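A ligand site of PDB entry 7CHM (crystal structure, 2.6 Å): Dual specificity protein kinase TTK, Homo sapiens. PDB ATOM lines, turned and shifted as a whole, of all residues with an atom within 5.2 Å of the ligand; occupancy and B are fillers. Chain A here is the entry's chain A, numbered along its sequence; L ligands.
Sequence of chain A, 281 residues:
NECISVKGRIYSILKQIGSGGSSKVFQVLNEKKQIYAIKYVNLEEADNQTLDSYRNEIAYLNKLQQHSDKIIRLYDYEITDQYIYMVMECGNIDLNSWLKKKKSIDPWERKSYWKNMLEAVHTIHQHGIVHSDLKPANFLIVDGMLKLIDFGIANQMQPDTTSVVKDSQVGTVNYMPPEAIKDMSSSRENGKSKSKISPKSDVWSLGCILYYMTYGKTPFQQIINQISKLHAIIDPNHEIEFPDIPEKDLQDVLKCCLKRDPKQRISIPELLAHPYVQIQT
The backbone carbonyl oxygen (O) of Glu 89 lies within hydrogen-bond range of a nitrogen (N5) of the ligand. The backbone NH of Gly 91 sits at hydrogen-bond distance from a nitrogen (N3) of the ligand (2.9 Å). N2 of the ligand lies close to O of Gly 91, at 3.0 Å. O1 of the ligand lies within hydrogen-bond range of SG of Cys 90 (3.6 Å).
Residues that only touch the ligand: Pro 159 (2.9 Å), Leu 140 (3.2 Å), Met 88 (3.2 Å), Ala 37 (3.4 Å), Ile 17 (3.5 Å), Ile 93 (3.5 Å), Ile 149 (3.5 Å), Asp 94 (3.5 Å), Asn 92 (3.5 Å), Gln 27 (3.6 Å), Val 25 (3.9 Å), Gln 158 (3.9 Å), Gly 18 (3.99 Å) and Ser 97 (3.99 Å). Hydrophobic or aromatic side chains within 4 Å of the ligand: Ile 17, Val 25, Ala 37, Met 88, Ile 93, Leu 140, Ile 149 and Pro 159. Of the 24 residues printed, 17 come within 4 Å of the ligand. Along chain A the residues within 4 Å of the ligand span positions 17 to 159. The nearest printed residue that does not touch the ligand is Lys 39 (4.01 Å).
The backbone NH (N) of Ala 37 sits at hydrogen-bond distance from the backbone carbonyl oxygen (O) of Met 88. The backbone NH (N) of Ile 17 is in hydrogen-bond range of the backbone carbonyl oxygen (O) of Val 25 (2.7 Å). The backbone carbonyl oxygen (O) of Ile 17 sits at hydrogen-bond distance from the backbone NH (N) of Asp 160, 2.8 Å away. The side-chain carboxylate (OD1) of Asp 94 is in hydrogen-bond range of the side-chain hydroxyl (OG) of Ser 97, at 2.7 Å. N of Gln 27 sits at hydrogen-bond distance from O of Lys 15. The backbone NH of Val 25 is in hydrogen-bond range of the backbone carbonyl oxygen of Gly 18 (3.0 Å).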
ATOM      1  N   LYS A  15      32.476  -6.384  -6.534  1.00  0.00           N
ATOM      2  CA  LYS A  15      31.923  -7.342  -5.585  1.00  0.00           C
ATOM      3  C   LYS A  15      30.849  -8.143  -6.293  1.00  0.00           C
ATOM      4  O   LYS A  15      30.435  -7.811  -7.406  1.00  0.00           O
ATOM      5  CB  LYS A  15      31.360  -6.634  -4.337  1.00  0.00           C
ATOM      6  CG  LYS A  15      29.858  -6.266  -4.401  1.00  0.00           C
ATOM      7  CD  LYS A  15      29.537  -5.044  -3.526  1.00  0.00           C
ATOM      8  CE  LYS A  15      28.048  -4.664  -3.502  1.00  0.00           C
ATOM      9  NZ  LYS A  15      27.796  -3.464  -2.633  1.00  0.00           N
ATOM     10  N   ILE A  17      27.146  -9.272  -6.348  1.00  0.00           N
ATOM     11  CA  ILE A  17      25.832  -8.932  -5.848  1.00  0.00           C
ATOM     12  C   ILE A  17      25.019 -10.180  -5.557  1.00  0.00           C
ATOM     13  O   ILE A  17      24.321 -10.249  -4.537  1.00  0.00           O
ATOM     14  CB  ILE A  17      25.119  -8.026  -6.866  1.00  0.00           C
ATOM     15  CG1 ILE A  17      25.918  -6.758  -7.073  1.00  0.00           C
ATOM     16  CG2 ILE A  17      23.687  -7.762  -6.442  1.00  0.00           C
ATOM     17  CD1 ILE A  17      25.597  -6.105  -8.399  1.00  0.00           C
ATOM     18  N   GLY A  18      25.057 -11.161  -6.452  1.00  0.00           N
ATOM     19  CA  GLY A  18      24.048 -12.203  -6.403  1.00  0.00           C
ATOM     20  C   GLY A  18      24.478 -13.522  -7.012  1.00  0.00           C
ATOM     21  O   GLY A  18      25.436 -13.581  -7.790  1.00  0.00           O
ATOM     22  N   VAL A  25      26.140 -12.390 -10.463  1.00  0.00           N
ATOM     23  CA  VAL A  25      26.063 -11.003 -10.867  1.00  0.00           C
ATOM     24  C   VAL A  25      27.089 -10.227 -10.066  1.00  0.00           C
ATOM     25  O   VAL A  25      27.182 -10.396  -8.837  1.00  0.00           O
ATOM     26  CB  VAL A  25      24.656 -10.420 -10.653  1.00  0.00           C
ATOM     27  CG1 VAL A  25      24.509  -9.057 -11.345  1.00  0.00           C
ATOM     28  CG2 VAL A  25      23.611 -11.381 -11.161  1.00  0.00           C
ATOM     29  N   GLN A  27      28.943  -6.369  -9.408  1.00  0.00           N
ATOM     30  CA  GLN A  27      29.242  -4.969  -9.637  1.00  0.00           C
ATOM     31  C   GLN A  27      30.672  -4.868 -10.147  1.00  0.00           C
ATOM     32  O   GLN A  27      31.578  -5.513  -9.604  1.00  0.00           O
ATOM     33  CB  GLN A  27      29.059  -4.235  -8.330  1.00  0.00           C
ATOM     34  CG  GLN A  27      29.154  -2.767  -8.349  1.00  0.00           C
ATOM     35  CD  GLN A  27      28.869  -2.260  -6.967  1.00  0.00           C
ATOM     36  OE1 GLN A  27      29.023  -3.008  -5.983  1.00  0.00           O
ATOM     37  NE2 GLN A  27      28.418  -1.008  -6.862  1.00  0.00           N
ATOM     38  N   ALA A  37      26.802  -3.674 -14.050  1.00  0.00           N
ATOM     39  CA  ALA A  37      26.624  -5.044 -13.574  1.00  0.00           C
ATOM     40  C   ALA A  37      27.010  -6.033 -14.670  1.00  0.00           C
ATOM     41  O   ALA A  37      26.944  -5.735 -15.864  1.00  0.00           O
ATOM     42  CB  ALA A  37      25.190  -5.292 -13.079  1.00  0.00           C
ATOM     43  N   LYS A  39      26.303 -10.170 -15.411  1.00  0.00           N
ATOM     44  CA  LYS A  39      25.776 -11.498 -15.151  1.00  0.00           C
ATOM     45  C   LYS A  39      26.658 -12.526 -15.859  1.00  0.00           C
ATOM     46  O   LYS A  39      27.040 -12.354 -17.016  1.00  0.00           O
ATOM     47  CB  LYS A  39      24.316 -11.612 -15.625  1.00  0.00           C
ATOM     48  CG  LYS A  39      23.480 -12.755 -15.029  1.00  0.00           C
ATOM     49  CD  LYS A  39      21.958 -12.556 -15.304  1.00  0.00           C
ATOM     50  CE  LYS A  39      21.097 -13.686 -14.720  1.00  0.00           C
ATOM     51  NZ  LYS A  39      19.698 -13.755 -15.244  1.00  0.00           N
ATOM     52  N   ILE A  72      15.829  -2.897 -17.582  1.00  0.00           N
ATOM     53  CA  ILE A  72      17.279  -2.750 -17.452  1.00  0.00           C
ATOM     54  C   ILE A  72      17.926  -2.637 -18.821  1.00  0.00           C
ATOM     55  O   ILE A  72      17.557  -3.347 -19.753  1.00  0.00           O
ATOM     56  CB  ILE A  72      17.858  -3.962 -16.699  1.00  0.00           C
ATOM     57  CG1 ILE A  72      17.254  -4.038 -15.305  1.00  0.00           C
ATOM     58  CG2 ILE A  72      19.349  -3.807 -16.539  1.00  0.00           C
ATOM     59  CD1 ILE A  72      17.530  -2.769 -14.477  1.00  0.00           C
ATOM     60  N   MET A  88      25.316  -5.021 -18.110  1.00  0.00           N
ATOM     61  CA  MET A  88      24.056  -4.325 -17.911  1.00  0.00           C
ATOM     62  C   MET A  88      24.269  -3.094 -17.055  1.00  0.00           C
ATOM     63  O   MET A  88      25.277  -2.960 -16.353  1.00  0.00           O
ATOM     64  CB  MET A  88      23.003  -5.209 -17.252  1.00  0.00           C
ATOM     65  CG  MET A  88      22.691  -6.405 -18.064  1.00  0.00           C
ATOM     66  SD  MET A  88      21.869  -7.654 -17.111  1.00  0.00           S
ATOM     67  CE  MET A  88      23.094  -7.982 -15.861  1.00  0.00           C
ATOM     68  N   GLU A  89      23.278  -2.196 -17.122  1.00  0.00           N
ATOM     69  CA  GLU A  89      23.271  -1.056 -16.220  1.00  0.00           C
ATOM     70  C   GLU A  89      23.121  -1.574 -14.805  1.00  0.00           C
ATOM     71  O   GLU A  89      22.415  -2.562 -14.564  1.00  0.00           O
ATOM     72  CB  GLU A  89      22.169  -0.059 -16.591  1.00  0.00           C
ATOM     73  CG  GLU A  89      20.925  -0.070 -15.723  1.00  0.00           C
ATOM     74  CD  GLU A  89      19.809   0.822 -16.285  1.00  0.00           C
ATOM     75  OE1 GLU A  89      19.441   1.846 -15.636  1.00  0.00           O
ATOM     76  OE2 GLU A  89      19.305   0.516 -17.391  1.00  0.00           O
ATOM     77  N   CYS A  90      23.861  -0.976 -13.889  1.00  0.00           N
ATOM     78  CA  CYS A  90      23.913  -1.446 -12.518  1.00  0.00           C
ATOM     79  C   CYS A  90      22.887  -0.702 -11.686  1.00  0.00           C
ATOM     80  O   CYS A  90      22.801   0.532 -11.759  1.00  0.00           O
ATOM     81  CB  CYS A  90      25.303  -1.253 -11.922  1.00  0.00           C
ATOM     82  SG  CYS A  90      25.476  -2.101 -10.338  1.00  0.00           S
ATOM     83  N   GLY A  91      22.106  -1.428 -10.910  1.00  0.00           N
ATOM     84  CA  GLY A  91      21.176  -0.767 -10.019  1.00  0.00           C
ATOM     85  C   GLY A  91      21.841  -0.302  -8.728  1.00  0.00           C
ATOM     86  O   GLY A  91      22.860  -0.847  -8.294  1.00  0.00           O
ATOM     87  N   ASN A  92      21.252   0.747  -8.142  1.00  0.00           N
ATOM     88  CA  ASN A  92      21.589   1.122  -6.762  1.00  0.00           C
ATOM     89  C   ASN A  92      21.256  -0.007  -5.790  1.00  0.00           C
ATOM     90  O   ASN A  92      22.037  -0.339  -4.892  1.00  0.00           O
ATOM     91  CB  ASN A  92      20.846   2.391  -6.371  1.00  0.00           C
ATOM     92  CG  ASN A  92      21.119   3.528  -7.318  1.00  0.00           C
ATOM     93  OD1 ASN A  92      21.667   3.308  -8.396  1.00  0.00           O
ATOM     94  ND2 ASN A  92      20.788   4.745  -6.913  1.00  0.00           N
ATOM     95  N   ILE A  93      20.127  -0.663  -6.000  1.00  0.00           N
ATOM     96  CA  ILE A  93      19.702  -1.733  -5.115  1.00  0.00           C
ATOM     97  C   ILE A  93      18.410  -2.295  -5.686  1.00  0.00           C
ATOM     98  O   ILE A  93      17.820  -1.694  -6.590  1.00  0.00           O
ATOM     99  CB  ILE A  93      19.523  -1.187  -3.687  1.00  0.00           C
ATOM    100  CG1 ILE A  93      19.081  -2.290  -2.730  1.00  0.00           C
ATOM    101  CG2 ILE A  93      18.564   0.018  -3.707  1.00  0.00           C
ATOM    102  CD1 ILE A  93      19.009  -1.847  -1.302  1.00  0.00           C
ATOM    103  N   ASP A  94      17.970  -3.436  -5.194  1.00  0.00           N
ATOM    104  CA  ASP A  94      16.678  -3.942  -5.613  1.00  0.00           C
ATOM    105  C   ASP A  94      15.580  -3.510  -4.643  1.00  0.00           C
ATOM    106  O   ASP A  94      15.826  -3.286  -3.459  1.00  0.00           O
ATOM    107  CB  ASP A  94      16.688  -5.457  -5.695  1.00  0.00           C
ATOM    108  CG  ASP A  94      16.999  -6.071  -4.383  1.00  0.00           C
ATOM    109  OD1 ASP A  94      18.063  -5.739  -3.840  1.00  0.00           O
ATOM    110  OD2 ASP A  94      16.185  -6.878  -3.886  1.00  0.00           O
ATOM    111  N   SER A  97      15.354  -5.546  -1.119  1.00  0.00           N
ATOM    112  CA  SER A  97      16.270  -5.113  -0.062  1.00  0.00           C
ATOM    113  C   SER A  97      15.947  -3.709   0.400  1.00  0.00           C
ATOM    114  O   SER A  97      15.893  -3.438   1.601  1.00  0.00           O
ATOM    115  CB  SER A  97      17.717  -5.200  -0.547  1.00  0.00           C
ATOM    116  OG  SER A  97      17.954  -6.436  -1.208  1.00  0.00           O
ATOM    117  N   ALA A 137      12.165  -8.184  -5.703  1.00  0.00           N
ATOM    118  CA  ALA A 137      13.501  -8.493  -6.202  1.00  0.00           C
ATOM    119  C   ALA A 137      13.605  -8.431  -7.720  1.00  0.00           C
ATOM    120  O   ALA A 137      14.723  -8.480  -8.254  1.00  0.00           O
ATOM    121  CB  ALA A 137      13.928  -9.877  -5.715  1.00  0.00           C
ATOM    122  N   LEU A 140      14.720  -2.901  -9.917  1.00  0.00           N
ATOM    123  CA  LEU A 140      15.950  -2.243  -9.524  1.00  0.00           C
ATOM    124  C   LEU A 140      15.672  -0.771  -9.440  1.00  0.00           C
ATOM    125  O   LEU A 140      15.085  -0.200 -10.365  1.00  0.00           O
ATOM    126  CB  LEU A 140      17.068  -2.471 -10.547  1.00  0.00           C
ATOM    127  CG  LEU A 140      17.712  -3.856 -10.521  1.00  0.00           C
ATOM    128  CD1 LEU A 140      18.978  -3.898 -11.381  1.00  0.00           C
ATOM    129  CD2 LEU A 140      18.006  -4.326  -9.101  1.00  0.00           C
ATOM    130  N   ILE A 149      14.096  -6.340 -14.175  1.00  0.00           N
ATOM    131  CA  ILE A 149      15.257  -7.156 -14.564  1.00  0.00           C
ATOM    132  C   ILE A 149      14.877  -8.507 -15.153  1.00  0.00           C
ATOM    133  O   ILE A 149      15.133  -8.774 -16.328  1.00  0.00           O
ATOM    134  CB  ILE A 149      16.200  -7.450 -13.389  1.00  0.00           C
ATOM    135  CG1 ILE A 149      16.548  -6.221 -12.618  1.00  0.00           C
ATOM    136  CG2 ILE A 149      17.473  -8.148 -13.900  1.00  0.00           C
ATOM    137  CD1 ILE A 149      16.887  -6.600 -11.197  1.00  0.00           C
ATOM    138  N   GLN A 156      15.906 -16.925 -11.975  1.00  0.00           N
ATOM    139  CA  GLN A 156      16.275 -15.742 -11.216  1.00  0.00           C
ATOM    140  C   GLN A 156      17.236 -16.116 -10.104  1.00  0.00           C
ATOM    141  O   GLN A 156      17.401 -17.297  -9.757  1.00  0.00           O
ATOM    142  CB  GLN A 156      15.039 -15.012 -10.647  1.00  0.00           C
ATOM    143  CG  GLN A 156      15.173 -13.442 -10.608  1.00  0.00           C
ATOM    144  CD  GLN A 156      15.357 -12.834  -9.201  1.00  0.00           C
ATOM    145  OE1 GLN A 156      15.215 -13.511  -8.184  1.00  0.00           O
ATOM    146  NE2 GLN A 156      15.679 -11.540  -9.147  1.00  0.00           N
ATOM    147  N   MET A 157      17.870 -15.093  -9.539  1.00  0.00           N
ATOM    148  CA  MET A 157      18.965 -15.228  -8.597  1.00  0.00           C
ATOM    149  C   MET A 157      18.557 -14.721  -7.227  1.00  0.00           C
ATOM    150  O   MET A 157      17.520 -14.060  -7.059  1.00  0.00           O
ATOM    151  CB  MET A 157      20.178 -14.445  -9.102  1.00  0.00           C
ATOM    152  CG  MET A 157      20.346 -14.559 -10.598  1.00  0.00           C
ATOM    153  SD  MET A 157      22.076 -14.531 -11.067  1.00  0.00           S
ATOM    154  CE  MET A 157      22.763 -15.777  -9.979  1.00  0.00           C
ATOM    155  N   GLN A 158      19.385 -15.043  -6.232  1.00  0.00           N
ATOM    156  CA  GLN A 158      19.258 -14.561  -4.870  1.00  0.00           C
ATOM    157  C   GLN A 158      20.430 -13.669  -4.495  1.00  0.00           C
ATOM    158  O   GLN A 158      21.521 -13.769  -5.086  1.00  0.00           O
ATOM    159  CB  GLN A 158      19.177 -15.728  -3.872  1.00  0.00           C
ATOM    160  CG  GLN A 158      17.761 -16.180  -3.501  1.00  0.00           C
ATOM    161  CD  GLN A 158      17.148 -17.090  -4.558  1.00  0.00           C
ATOM    162  OE1 GLN A 158      17.866 -17.763  -5.320  1.00  0.00           O
ATOM    163  NE2 GLN A 158      15.813 -17.113  -4.604  1.00  0.00           N
ATOM    164  N   PRO A 159      20.252 -12.799  -3.519  1.00  0.00           N
ATOM    165  CA  PRO A 159      21.344 -11.888  -3.118  1.00  0.00           C
ATOM    166  C   PRO A 159      22.485 -12.623  -2.403  1.00  0.00           C
ATOM    167  O   PRO A 159      22.279 -13.651  -1.761  1.00  0.00           O
ATOM    168  CB  PRO A 159      20.651 -10.898  -2.191  1.00  0.00           C
ATOM    169  CG  PRO A 159      19.463 -11.628  -1.667  1.00  0.00           C
ATOM    170  CD  PRO A 159      19.021 -12.568  -2.742  1.00  0.00           C
ATOM    171  N   ASP A 160      23.684 -12.059  -2.499  1.00  0.00           N
ATOM    172  CA  ASP A 160      24.847 -12.621  -1.795  1.00  0.00           C
ATOM    173  C   ASP A 160      25.465 -11.713  -0.724  1.00  0.00           C
ATOM    174  O   ASP A 160      25.876 -10.576  -1.014  1.00  0.00           O
ATOM    175  CB  ASP A 160      25.937 -13.010  -2.786  1.00  0.00           C
ATOM    176  CG  ASP A 160      25.843 -14.475  -3.204  1.00  0.00           C
ATOM    177  OD1 ASP A 160      26.123 -15.373  -2.388  1.00  0.00           O
ATOM    178  OD2 ASP A 160      25.482 -14.707  -4.366  1.00  0.00           O
HETATM  179  C1  LIG L   1      21.249  -4.822  -6.575  1.00  0.00           C
HETATM  180  C2  LIG L   1      21.854  -5.147 -11.874  1.00  0.00           C
HETATM  181  C3  LIG L   1      21.494  -6.433 -11.584  1.00  0.00           C
HETATM  182  C4  LIG L   1      21.258  -7.068 -12.812  1.00  0.00           C
HETATM  183  C5  LIG L   1      24.909  -1.816  -6.359  1.00  0.00           C
HETATM  184  C6  LIG L   1      23.365  -3.642  -6.366  1.00  0.00           C
HETATM  185  C7  LIG L   1      23.389  -3.868  -5.009  1.00  0.00           C
HETATM  186  C8  LIG L   1      22.333  -4.547  -4.448  1.00  0.00           C
HETATM  187  C9  LIG L   1      22.377  -4.722  -2.924  1.00  0.00           C
HETATM  188  C10 LIG L   1      22.715  -6.231  -0.932  1.00  0.00           C
HETATM  189  C11 LIG L   1      21.777  -7.352  -0.515  1.00  0.00           C
HETATM  190  C12 LIG L   1      21.986  -8.280  -2.690  1.00  0.00           C
HETATM  191  C13 LIG L   1      22.900  -7.148  -3.118  1.00  0.00           C
HETATM  192  C14 LIG L   1      21.259  -5.039  -5.204  1.00  0.00           C
HETATM  193  C15 LIG L   1      22.315  -4.133  -7.140  1.00  0.00           C
HETATM  194  C16 LIG L   1      22.027  -4.758  -9.594  1.00  0.00           C
HETATM  195  C17 LIG L   1      20.835  -8.519 -12.945  1.00  0.00           C
HETATM  196  C18 LIG L   1      21.461  -6.127 -13.816  1.00  0.00           C
HETATM  197  C19 LIG L   1      21.421  -6.844 -10.210  1.00  0.00           C
HETATM  198  C20 LIG L   1      20.744  -8.449  -8.431  1.00  0.00           C
HETATM  199  C21 LIG L   1      19.356  -7.956  -8.135  1.00  0.00           C
HETATM  200  C22 LIG L   1      18.732  -8.541  -6.862  1.00  0.00           C
HETATM  201  C23 LIG L   1      19.112  -9.966  -6.430  1.00  0.00           C
HETATM  202  C24 LIG L   1      20.499 -10.439  -6.837  1.00  0.00           C
HETATM  203  C25 LIG L   1      20.902  -9.947  -8.218  1.00  0.00           C
HETATM  204  N1  LIG L   1      22.650  -5.989  -2.340  1.00  0.00           N
HETATM  205  N2  LIG L   1      22.371  -3.824  -8.564  1.00  0.00           N
HETATM  206  N3  LIG L   1      22.109  -4.323 -10.823  1.00  0.00           N
HETATM  207  N4  LIG L   1      20.532  -9.610 -12.991  1.00  0.00           N
HETATM  208  N5  LIG L   1      21.841  -4.971 -13.249  1.00  0.00           N
HETATM  209  N6  LIG L   1      21.042  -8.187  -9.827  1.00  0.00           N
HETATM  210  N7  LIG L   1      21.700  -5.982  -9.263  1.00  0.00           N
HETATM  211  O1  LIG L   1      24.425  -2.956  -6.997  1.00  0.00           O
HETATM  212  O2  LIG L   1      22.040  -8.514  -1.292  1.00  0.00           O
HETATM  213  O3  LIG L   1      22.183  -3.776  -2.239  1.00  0.00           O
